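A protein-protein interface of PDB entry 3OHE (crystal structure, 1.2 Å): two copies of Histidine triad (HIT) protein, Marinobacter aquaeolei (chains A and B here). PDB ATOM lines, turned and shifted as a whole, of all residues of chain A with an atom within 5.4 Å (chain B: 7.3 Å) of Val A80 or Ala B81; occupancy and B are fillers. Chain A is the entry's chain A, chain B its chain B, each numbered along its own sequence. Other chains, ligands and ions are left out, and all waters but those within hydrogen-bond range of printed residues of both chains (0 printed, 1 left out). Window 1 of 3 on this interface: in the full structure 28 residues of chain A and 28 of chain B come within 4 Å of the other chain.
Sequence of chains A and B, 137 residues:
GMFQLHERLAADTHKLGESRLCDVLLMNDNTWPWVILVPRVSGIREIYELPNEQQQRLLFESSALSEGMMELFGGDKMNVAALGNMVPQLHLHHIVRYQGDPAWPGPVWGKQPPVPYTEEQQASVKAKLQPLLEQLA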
ATOM      1  N   SER A  62     -13.855 -19.842  -0.067  1.00  0.00           N
ATOM      2  CA  SER A  62     -13.431 -20.611   1.099  1.00  0.00           C
ATOM      3  C   SER A  62     -14.616 -21.254   1.799  1.00  0.00           C
ATOM      4  O   SER A  62     -14.576 -22.437   2.162  1.00  0.00           O
ATOM      5  CB  SER A  62     -12.695 -19.714   2.074  1.00  0.00           C
ATOM      6  OG  SER A  62     -12.324 -20.415   3.247  1.00  0.00           O
ATOM      7  N   SER A  66     -15.219 -25.206   1.956  1.00  0.00           N
ATOM      8  CA  SER A  66     -15.252 -25.849   3.284  1.00  0.00           C
ATOM      9  C   SER A  66     -16.523 -26.676   3.443  1.00  0.00           C
ATOM     10  O   SER A  66     -16.461 -27.860   3.788  1.00  0.00           O
ATOM     11  CB  SER A  66     -15.213 -24.821   4.421  1.00  0.00           C
ATOM     12  OG  SER A  66     -13.988 -24.141   4.477  1.00  0.00           O
ATOM     13  N   MET A  78     -14.085 -28.780  10.360  1.00  0.00           N
ATOM     14  CA  MET A  78     -13.103 -28.122   9.506  1.00  0.00           C
ATOM     15  C   MET A  78     -12.089 -27.353  10.287  1.00  0.00           C
ATOM     16  O   MET A  78     -12.380 -26.819  11.357  1.00  0.00           O
ATOM     17  CB  MET A  78     -13.772 -27.140   8.531  1.00  0.00           C
ATOM     18  CG  MET A  78     -14.625 -27.814   7.502  1.00  0.00           C
ATOM     19  SD  MET A  78     -13.676 -29.051   6.317  1.00  0.00           S
ATOM     20  CE  MET A  78     -12.385 -27.986   5.431  1.00  0.00           C
ATOM     21  N   ASN A  79     -10.886 -27.290   9.733  1.00  0.00           N
ATOM     22  CA  ASN A  79      -9.857 -26.353  10.222  1.00  0.00           C
ATOM     23  C   ASN A  79      -9.442 -25.478   9.024  1.00  0.00           C
ATOM     24  O   ASN A  79      -9.074 -26.009   7.969  1.00  0.00           O
ATOM     25  CB  ASN A  79      -8.645 -27.081  10.763  1.00  0.00           C
ATOM     26  CG  ASN A  79      -8.853 -27.840  12.080  1.00  0.00           C
ATOM     27  OD1 ASN A  79      -7.868 -28.463  12.523  1.00  0.00           O
ATOM     28  ND2 ASN A  79     -10.021 -27.789  12.706  1.00  0.00           N
ATOM     29  N   VAL A  80      -9.549 -24.161   9.184  1.00  0.00           N
ATOM     30  CA  VAL A  80      -9.240 -23.205   8.143  1.00  0.00           C
ATOM     31  C   VAL A  80      -8.235 -22.226   8.718  1.00  0.00           C
ATOM     32  O   VAL A  80      -8.395 -21.735   9.841  1.00  0.00           O
ATOM     33  CB  VAL A  80     -10.508 -22.484   7.637  1.00  0.00           C
ATOM     34  CG1 VAL A  80     -10.171 -21.477   6.508  1.00  0.00           C
ATOM     35  CG2 VAL A  80     -11.520 -23.509   7.075  1.00  0.00           C
ATOM     36  N   ALA A  81      -7.156 -21.948   7.974  1.00  0.00           N
ATOM     37  CA  ALA A  81      -6.063 -21.136   8.530  1.00  0.00           C
ATOM     38  C   ALA A  81      -5.248 -20.448   7.465  1.00  0.00           C
ATOM     39  O   ALA A  81      -4.989 -21.019   6.407  1.00  0.00           O
ATOM     40  CB  ALA A  81      -5.103 -21.982   9.421  1.00  0.00           C
ATOM     41  N   ALA A  82      -4.785 -19.234   7.775  1.00  0.00           N
ATOM     42  CA  ALA A  82      -3.793 -18.509   6.974  1.00  0.00           C
ATOM     43  C   ALA A  82      -2.629 -18.279   7.964  1.00  0.00           C
ATOM     44  O   ALA A  82      -2.777 -17.527   8.928  1.00  0.00           O
ATOM     45  CB  ALA A  82      -4.381 -17.163   6.451  1.00  0.00           C
ATOM     46  N   LEU A  83      -1.495 -18.954   7.738  1.00  0.00           N
ATOM     47  CA  LEU A  83      -0.350 -18.961   8.631  1.00  0.00           C
ATOM     48  C   LEU A  83       0.822 -18.266   7.881  1.00  0.00           C
ATOM     49  O   LEU A  83       1.050 -17.067   8.082  1.00  0.00           O
ATOM     50  CB  LEU A  83      -0.067 -20.395   9.076  1.00  0.00           C
ATOM     51  CG  LEU A  83      -1.228 -21.102   9.741  1.00  0.00           C
ATOM     52  CD1 LEU A  83      -0.876 -22.548  10.043  1.00  0.00           C
ATOM     53  CD2 LEU A  83      -1.736 -20.355  10.975  1.00  0.00           C
ATOM     54  N   LEU A  92      -4.572 -20.229   1.856  1.00  0.00           N
ATOM     55  CA  LEU A  92      -5.565 -20.526   2.875  1.00  0.00           C
ATOM     56  C   LEU A  92      -5.761 -22.037   2.950  1.00  0.00           C
ATOM     57  O   LEU A  92      -6.203 -22.659   1.977  1.00  0.00           O
ATOM     58  CB  LEU A  92      -6.856 -19.754   2.523  1.00  0.00           C
ATOM     59  CG  LEU A  92      -7.997 -19.720   3.517  1.00  0.00           C
ATOM     60  CD1 LEU A  92      -7.508 -19.035   4.828  1.00  0.00           C
ATOM     61  CD2 LEU A  92      -9.239 -18.986   2.965  1.00  0.00           C
ATOM     62  N   HIS A  93      -5.413 -22.615   4.095  1.00  0.00           N
ATOM     63  CA  HIS A  93      -5.546 -24.058   4.371  1.00  0.00           C
ATOM     64  C   HIS A  93      -6.963 -24.427   4.721  1.00  0.00           C
ATOM     65  O   HIS A  93      -7.592 -23.739   5.509  1.00  0.00           O
ATOM     66  CB  HIS A  93      -4.669 -24.441   5.570  1.00  0.00           C
ATOM     67  CG  HIS A  93      -3.217 -24.185   5.389  1.00  0.00           C
ATOM     68  ND1 HIS A  93      -2.414 -25.031   4.667  1.00  0.00           N
ATOM     69  CD2 HIS A  93      -2.429 -23.216   5.895  1.00  0.00           C
ATOM     70  CE1 HIS A  93      -1.182 -24.565   4.713  1.00  0.00           C
ATOM     71  NE2 HIS A  93      -1.163 -23.466   5.447  1.00  0.00           N
ATOM     72  N   HIS A  94      -7.439 -25.541   4.154  1.00  0.00           N
ATOM     73  CA  HIS A  94      -8.747 -26.130   4.465  1.00  0.00           C
ATOM     74  C   HIS A  94      -8.530 -27.619   4.729  1.00  0.00           C
ATOM     75  O   HIS A  94      -8.199 -28.360   3.802  1.00  0.00           O
ATOM     76  CB  HIS A  94      -9.730 -25.950   3.300  1.00  0.00           C
ATOM     77  CG  HIS A  94      -9.930 -24.536   2.882  1.00  0.00           C
ATOM     78  ND1 HIS A  94      -8.996 -23.831   2.164  1.00  0.00           N
ATOM     79  CD2 HIS A  94     -10.944 -23.686   3.119  1.00  0.00           C
ATOM     80  CE1 HIS A  94      -9.445 -22.597   1.984  1.00  0.00           C
ATOM     81  NE2 HIS A  94     -10.628 -22.481   2.546  1.00  0.00           N
ATOM     82  N   ILE A  95      -8.662 -28.006   5.995  1.00  0.00           N
ATOM     83  CA  ILE A  95      -8.298 -29.371   6.415  1.00  0.00           C
ATOM     84  C   ILE A  95      -9.515 -30.029   7.063  1.00  0.00           C
ATOM     85  O   ILE A  95     -10.086 -29.485   8.012  1.00  0.00           O
ATOM     86  CB  ILE A  95      -7.123 -29.365   7.389  1.00  0.00           C
ATOM     87  CG1 ILE A  95      -5.957 -28.507   6.845  1.00  0.00           C
ATOM     88  CG2 ILE A  95      -6.662 -30.812   7.661  1.00  0.00           C
ATOM     89  CD1 ILE A  95      -4.851 -28.243   7.832  1.00  0.00           C
ATOM     90  N   ILE B  36      -9.199 -13.254  20.050  1.00  0.00           N
ATOM     91  CA  ILE B  36     -10.187 -14.175  19.487  1.00  0.00           C
ATOM     92  C   ILE B  36     -11.494 -13.424  19.274  1.00  0.00           C
ATOM     93  O   ILE B  36     -11.968 -12.717  20.181  1.00  0.00           O
ATOM     94  CB  ILE B  36     -10.404 -15.380  20.423  1.00  0.00           C
ATOM     95  CG1 ILE B  36      -9.099 -16.173  20.607  1.00  0.00           C
ATOM     96  CG2 ILE B  36     -11.523 -16.285  19.936  1.00  0.00           C
ATOM     97  CD1 ILE B  36      -9.131 -17.283  21.659  1.00  0.00           C
ATOM     98  N   GLU B  46     -18.994 -23.378  12.246  1.00  0.00           N
ATOM     99  CA  GLU B  46     -18.135 -23.079  11.117  1.00  0.00           C
ATOM    100  C   GLU B  46     -18.516 -21.713  10.561  1.00  0.00           C
ATOM    101  O   GLU B  46     -19.692 -21.344  10.596  1.00  0.00           O
ATOM    102  CB  GLU B  46     -18.313 -24.160  10.024  1.00  0.00           C
ATOM    103  CG  GLU B  46     -18.076 -25.588  10.447  1.00  0.00           C
ATOM    104  CD  GLU B  46     -16.598 -25.923  10.687  1.00  0.00           C
ATOM    105  OE1 GLU B  46     -15.721 -25.045  10.477  1.00  0.00           O
ATOM    106  OE2 GLU B  46     -16.346 -27.064  11.128  1.00  0.00           O
ATOM    107  N   ILE B  47     -17.547 -21.030   9.957  1.00  0.00           N
ATOM    108  CA  ILE B  47     -17.810 -19.733   9.343  1.00  0.00           C
ATOM    109  C   ILE B  47     -18.955 -19.830   8.330  1.00  0.00           C
ATOM    110  O   ILE B  47     -19.805 -18.945   8.247  1.00  0.00           O
ATOM    111  CB  ILE B  47     -16.530 -19.172   8.669  1.00  0.00           C
ATOM    112  CG1 ILE B  47     -15.446 -18.864   9.709  1.00  0.00           C
ATOM    113  CG2 ILE B  47     -16.864 -17.900   7.817  1.00  0.00           C
ATOM    114  CD1 ILE B  47     -14.082 -18.662   9.052  1.00  0.00           C
ATOM    115  N   TYR B  48     -18.960 -20.900   7.540  1.00  0.00           N
ATOM    116  CA  TYR B  48     -19.925 -21.017   6.446  1.00  0.00           C
ATOM    117  C   TYR B  48     -21.374 -21.203   6.908  1.00  0.00           C
ATOM    118  O   TYR B  48     -22.294 -21.075   6.109  1.00  0.00           O
ATOM    119  CB  TYR B  48     -19.536 -22.121   5.476  1.00  0.00           C
ATOM    120  CG  TYR B  48     -19.490 -23.513   6.090  1.00  0.00           C
ATOM    121  CD1 TYR B  48     -20.652 -24.235   6.343  1.00  0.00           C
ATOM    122  CD2 TYR B  48     -18.282 -24.145   6.330  1.00  0.00           C
ATOM    123  CE1 TYR B  48     -20.596 -25.511   6.839  1.00  0.00           C
ATOM    124  CE2 TYR B  48     -18.206 -25.430   6.839  1.00  0.00           C
ATOM    125  CZ  TYR B  48     -19.378 -26.120   7.098  1.00  0.00           C
ATOM    126  OH  TYR B  48     -19.255 -27.406   7.581  1.00  0.00           O
ATOM    127  N   SER B  62     -12.289  -9.178  11.216  1.00  0.00           N
ATOM    128  CA  SER B  62     -11.029  -9.932  11.272  1.00  0.00           C
ATOM    129  C   SER B  62      -9.893  -9.183  10.560  1.00  0.00           C
ATOM    130  O   SER B  62      -8.795  -9.054  11.073  1.00  0.00           O
ATOM    131  CB  SER B  62     -11.217 -11.294  10.629  1.00  0.00           C
ATOM    132  OG  SER B  62     -10.012 -12.013  10.544  1.00  0.00           O
ATOM    133  N   ASN B  79      -1.082 -14.832  12.101  1.00  0.00           N
ATOM    134  CA  ASN B  79      -1.677 -16.162  11.916  1.00  0.00           C
ATOM    135  C   ASN B  79      -3.147 -16.035  12.296  1.00  0.00           C
ATOM    136  O   ASN B  79      -3.483 -15.547  13.386  1.00  0.00           O
ATOM    137  CB  ASN B  79      -0.986 -17.181  12.832  1.00  0.00           C
ATOM    138  CG  ASN B  79       0.451 -17.561  12.469  1.00  0.00           C
ATOM    139  OD1 ASN B  79       1.051 -18.333  13.209  1.00  0.00           O
ATOM    140  ND2 ASN B  79       1.021 -17.055  11.352  1.00  0.00           N
ATOM    141  N   VAL B  80      -4.028 -16.468  11.392  1.00  0.00           N
ATOM    142  CA  VAL B  80      -5.474 -16.332  11.587  1.00  0.00           C
ATOM    143  C   VAL B  80      -6.043 -17.739  11.365  1.00  0.00           C
ATOM    144  O   VAL B  80      -5.693 -18.393  10.377  1.00  0.00           O
ATOM    145  CB  VAL B  80      -6.117 -15.310  10.644  1.00  0.00           C
ATOM    146  CG1 VAL B  80      -7.586 -15.217  10.878  1.00  0.00           C
ATOM    147  CG2 VAL B  80      -5.479 -13.936  10.875  1.00  0.00           C
ATOM    148  N   ALA B  81      -6.939 -18.213  12.229  1.00  0.00           N
ATOM    149  CA  ALA B  81      -7.468 -19.581  12.058  1.00  0.00           C
ATOM    150  C   ALA B  81      -8.782 -19.776  12.776  1.00  0.00           C
ATOM    151  O   ALA B  81      -9.006 -19.219  13.864  1.00  0.00           O
ATOM    152  CB  ALA B  81      -6.466 -20.607  12.599  1.00  0.00           C
ATOM    153  N   ALA B  82      -9.609 -20.650  12.209  1.00  0.00           N
ATOM    154  CA  ALA B  82     -10.772 -21.209  12.888  1.00  0.00           C
ATOM    155  C   ALA B  82     -10.540 -22.714  12.935  1.00  0.00           C
ATOM    156  O   ALA B  82     -10.504 -23.368  11.899  1.00  0.00           O
ATOM    157  CB  ALA B  82     -12.038 -20.862  12.103  1.00  0.00           C
ATOM    158  N   LEU B  83     -10.370 -23.230  14.154  1.00  0.00           N
ATOM    159  CA  LEU B  83      -9.995 -24.638  14.381  1.00  0.00           C
ATOM    160  C   LEU B  83     -11.169 -25.325  15.085  1.00  0.00           C
ATOM    161  O   LEU B  83     -12.020 -25.957  14.436  1.00  0.00           O
ATOM    162  CB  LEU B  83      -8.648 -24.714  15.136  1.00  0.00           C
ATOM    163  CG  LEU B  83      -7.474 -23.981  14.461  1.00  0.00           C
ATOM    164  CD1 LEU B  83      -6.237 -24.050  15.338  1.00  0.00           C
ATOM    165  CD2 LEU B  83      -7.192 -24.513  13.038  1.00  0.00           C
ATOM    166  N   GLY B  84     -11.270 -25.188  16.402  1.00  0.00           N
ATOM    167  CA  GLY B  84     -12.462 -25.608  17.127  1.00  0.00           C
ATOM    168  C   GLY B  84     -12.654 -27.096  17.281  1.00  0.00           C
ATOM    169  O   GLY B  84     -13.774 -27.574  17.368  1.00  0.00           O
ATOM    170  N   LEU B  90     -17.950 -21.418  17.186  1.00  0.00           N
ATOM    171  CA  LEU B  90     -17.072 -20.738  16.241  1.00  0.00           C
ATOM    172  C   LEU B  90     -16.330 -19.590  16.902  1.00  0.00           C
ATOM    173  O   LEU B  90     -16.934 -18.698  17.494  1.00  0.00           O
ATOM    174  CB  LEU B  90     -17.886 -20.212  15.054  1.00  0.00           C
ATOM    175  CG  LEU B  90     -17.136 -19.262  14.087  1.00  0.00           C
ATOM    176  CD1 LEU B  90     -15.984 -19.988  13.372  1.00  0.00           C
ATOM    177  CD2 LEU B  90     -18.126 -18.670  13.100  1.00  0.00           C
ATOM    178  N   HIS B  91     -15.022 -19.597  16.725  1.00  0.00           N
ATOM    179  CA  HIS B  91     -14.185 -18.532  17.220  1.00  0.00           C
ATOM    180  C   HIS B  91     -12.954 -18.421  16.332  1.00  0.00           C
ATOM    181  O   HIS B  91     -12.403 -19.415  15.873  1.00  0.00           O
ATOM    182  CB  HIS B  91     -13.831 -18.744  18.713  1.00  0.00           C
ATOM    183  CG  HIS B  91     -13.062 -19.999  19.045  1.00  0.00           C
ATOM    184  ND1 HIS B  91     -13.642 -21.257  19.107  1.00  0.00           N
ATOM    185  CD2 HIS B  91     -11.763 -20.183  19.401  1.00  0.00           C
ATOM    186  CE1 HIS B  91     -12.734 -22.153  19.494  1.00  0.00           C
ATOM    187  NE2 HIS B  91     -11.587 -21.522  19.679  1.00  0.00           N
ATOM    188  N   LEU B  92     -12.516 -17.200  16.077  1.00  0.00           N
ATOM    189  CA  LEU B  92     -11.494 -16.933  15.081  1.00  0.00           C
ATOM    190  C   LEU B  92     -10.258 -16.341  15.768  1.00  0.00           C
ATOM    191  O   LEU B  92     -10.307 -15.224  16.334  1.00  0.00           O
ATOM    192  CB  LEU B  92     -12.072 -16.010  14.005  1.00  0.00           C
ATOM    193  CG  LEU B  92     -11.224 -15.717  12.770  1.00  0.00           C
ATOM    194  CD1 LEU B  92     -11.024 -17.010  11.966  1.00  0.00           C
ATOM    195  CD2 LEU B  92     -11.859 -14.629  11.901  1.00  0.00           C
ATOM    196  N   HIS B  93      -9.160 -17.099  15.724  1.00  0.00           N
ATOM    197  CA  HIS B  93      -7.883 -16.722  16.353  1.00  0.00           C
ATOM    198  C   HIS B  93      -7.121 -15.731  15.509  1.00  0.00           C
ATOM    199  O   HIS B  93      -7.046 -15.895  14.293  1.00  0.00           O
ATOM    200  CB  HIS B  93      -6.991 -17.949  16.488  1.00  0.00           C
ATOM    201  CG  HIS B  93      -7.544 -19.035  17.345  1.00  0.00           C
ATOM    202  ND1 HIS B  93      -7.445 -19.000  18.716  1.00  0.00           N
ATOM    203  CD2 HIS B  93      -8.098 -20.226  17.016  1.00  0.00           C
ATOM    204  CE1 HIS B  93      -7.956 -20.118  19.203  1.00  0.00           C
ATOM    205  NE2 HIS B  93      -8.390 -20.870  18.193  1.00  0.00           N
ATOM    206  N   HIS B  94      -6.522 -14.734  16.164  1.00  0.00           N
ATOM    207  CA  HIS B  94      -5.630 -13.740  15.529  1.00  0.00           C
ATOM    208  C   HIS B  94      -4.382 -13.623  16.386  1.00  0.00           C
ATOM    209  O   HIS B  94      -4.436 -13.096  17.496  1.00  0.00           O
ATOM    210  CB  HIS B  94      -6.321 -12.373  15.447  1.00  0.00           C
ATOM    211  CG  HIS B  94      -7.606 -12.404  14.688  1.00  0.00           C
ATOM    212  ND1 HIS B  94      -8.770 -12.915  15.230  1.00  0.00           N
ATOM    213  CD2 HIS B  94      -7.918 -12.044  13.418  1.00  0.00           C
ATOM    214  CE1 HIS B  94      -9.720 -12.867  14.308  1.00  0.00           C
ATOM    215  NE2 HIS B  94      -9.236 -12.338  13.211  1.00  0.00           N
ATOM    216  N   ILE B  95      -3.249 -14.122  15.878  1.00  0.00           N
ATOM    217  CA  ILE B  95      -2.003 -14.154  16.641  1.00  0.00           C
ATOM    218  C   ILE B  95      -0.916 -13.385  15.884  1.00  0.00           C
ATOM    219  O   ILE B  95      -0.667 -13.670  14.720  1.00  0.00           O
ATOM    220  CB  ILE B  95      -1.558 -15.595  16.926  1.00  0.00           C
ATOM    221  CG1 ILE B  95      -2.742 -16.429  17.445  1.00  0.00           C
ATOM    222  CG2 ILE B  95      -0.348 -15.597  17.882  1.00  0.00           C
ATOM    223  CD1 ILE B  95      -2.564 -17.905  17.465  1.00  0.00           C
ATOM    224  N   TRP B 109      -0.609 -23.275  18.511  1.00  0.00           N
ATOM    225  CA  TRP B 109      -1.639 -24.020  19.250  1.00  0.00           C
ATOM    226  C   TRP B 109      -1.050 -25.346  19.750  1.00  0.00           C
ATOM    227  O   TRP B 109      -0.363 -26.065  19.013  1.00  0.00           O
ATOM    228  CB  TRP B 109      -2.890 -24.281  18.391  1.00  0.00           C
ATOM    229  CG  TRP B 109      -3.507 -23.035  17.898  1.00  0.00           C
ATOM    230  CD1 TRP B 109      -4.297 -22.199  18.582  1.00  0.00           C
ATOM    231  CD2 TRP B 109      -3.315 -22.468  16.609  1.00  0.00           C
ATOM    232  NE1 TRP B 109      -4.629 -21.106  17.799  1.00  0.00           N
ATOM    233  CE2 TRP B 109      -4.051 -21.271  16.561  1.00  0.00           C
ATOM    234  CE3 TRP B 109      -2.654 -22.891  15.457  1.00  0.00           C
ATOM    235  CZ2 TRP B 109      -4.096 -20.474  15.440  1.00  0.00           C
ATOM    236  CZ3 TRP B 109      -2.703 -22.100  14.340  1.00  0.00           C
ATOM    237  CH2 TRP B 109      -3.407 -20.900  14.340  1.00  0.00           C
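O of Leu A83 is in hydrogen-bond range of ND2 of Asn B79, 3.3 Å away.
The backbone NH (N) of Ala A82 lies within hydrogen-bond range of the backbone carbonyl oxygen (O) of Val B80 (2.9 Å).
The side-chain carboxylate of Glu B46 is in hydrogen-bond range of the backbone NH of Met A78, 2.9 Å away.
The side-chain amide nitrogen (ND2) of Asn A79 lies within hydrogen-bond range of the backbone carbonyl oxygen (O) of Leu B83.
The backbone carbonyl oxygen of Met A78 sits close to the backbone carbonyl oxygen of Leu B83 (3.2 Å).
O of Val A80 lies within hydrogen-bond range of N of Ala B82 (2.9 Å).
Tyr B48 touches Ser A66.
Ala B82 touches Met A78.
O of Ala B82 touches CA of Asn A79, 3.5 Å away.
O of Val A80 touches CA of Ala B81, 3.2 Å away.
CA of Ala A81 touches O of Val B80, 3.3 Å away.
Ala B81 touches Ala A81 (CB to CB, 3.7 Å).
CA of Asn B79 touches O of Ala A82 (3.5 Å).
Trp B109 touches Leu A83 (CH2 to CD2, 3.8 Å).
Hydrophobic or aromatic side chains of chain B that line the printed part of chain A: Tyr B48, Ala B81, Leu B83 and Trp B109.
Hydrophobic or aromatic side chains of chain A within 4 Å of the printed part of chain B: Met A78, Ala A81 and Leu A83.
Asn A79 touches Ala B82, and with the chains exchanged Ala A82 touches Asn B79.
Asn A79 touches Leu B83, and with the chains exchanged Leu A83 touches Asn B79.
Val A80 touches Ala B81, and with the chains exchanged Ala A81 touches Val B80.
Ala B81 touches its own counterpart, Ala A81.
Positions printed for both chains: 62, 79, 80, 81, 82, 83, 92, 93, 94 and 95.
Of the 14 pairs that touch across the chains among the printed residues, 9 have their exchanged pair printed and touching as well.
Printed residues of chain B within 4 Å of Val A80: Ala B81 and Ala B82.
Of chain A, only Val A80 and Ala A81 come within 4 Å of Ala B81.
Of the printed residues of chain A, Ala B82 touches Met A78 (3.97 Å), Asn A79 (3.5 Å) and Val A80 (2.9 Å).
Printed residues of chain B within 4 Å of Asn A79: Ala B82 and Leu B83.
Of the printed residues of chain A, Leu B83 touches Met A78 (3.2 Å) and Asn A79 (3.2 Å).
Of the printed residues of chain B, Met A78 touches Glu B46 (2.9 Å), Ala B82 (3.97 Å) and Leu B83 (3.2 Å).
Of the printed residues of chain A, Glu B46 touches Met A78 (2.9 Å).
Ile B47 touches none of the printed residues of chain A.
The nearest residue of chain A that does not touch Ala B81 is Leu A83 (5.0 Å).
The nearest printed residue of chain B that does not touch Leu A83 is Val B80 (4.5 Å).
O of Ser A62 sits at hydrogen-bond distance from OG of Ser A66.
O of Asn B79 lies within hydrogen-bond range of N of Ile B95, 2.9 Å away.
The backbone NH (N) of Ile A95 is in hydrogen-bond range of the backbone carbonyl oxygen (O) of Asn A79.
The backbone carbonyl oxygen (O) of Ala B81 sits at hydrogen-bond distance from the backbone NH (N) of His B93.
O of Ala A81 lies within hydrogen-bond range of N of His A93.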
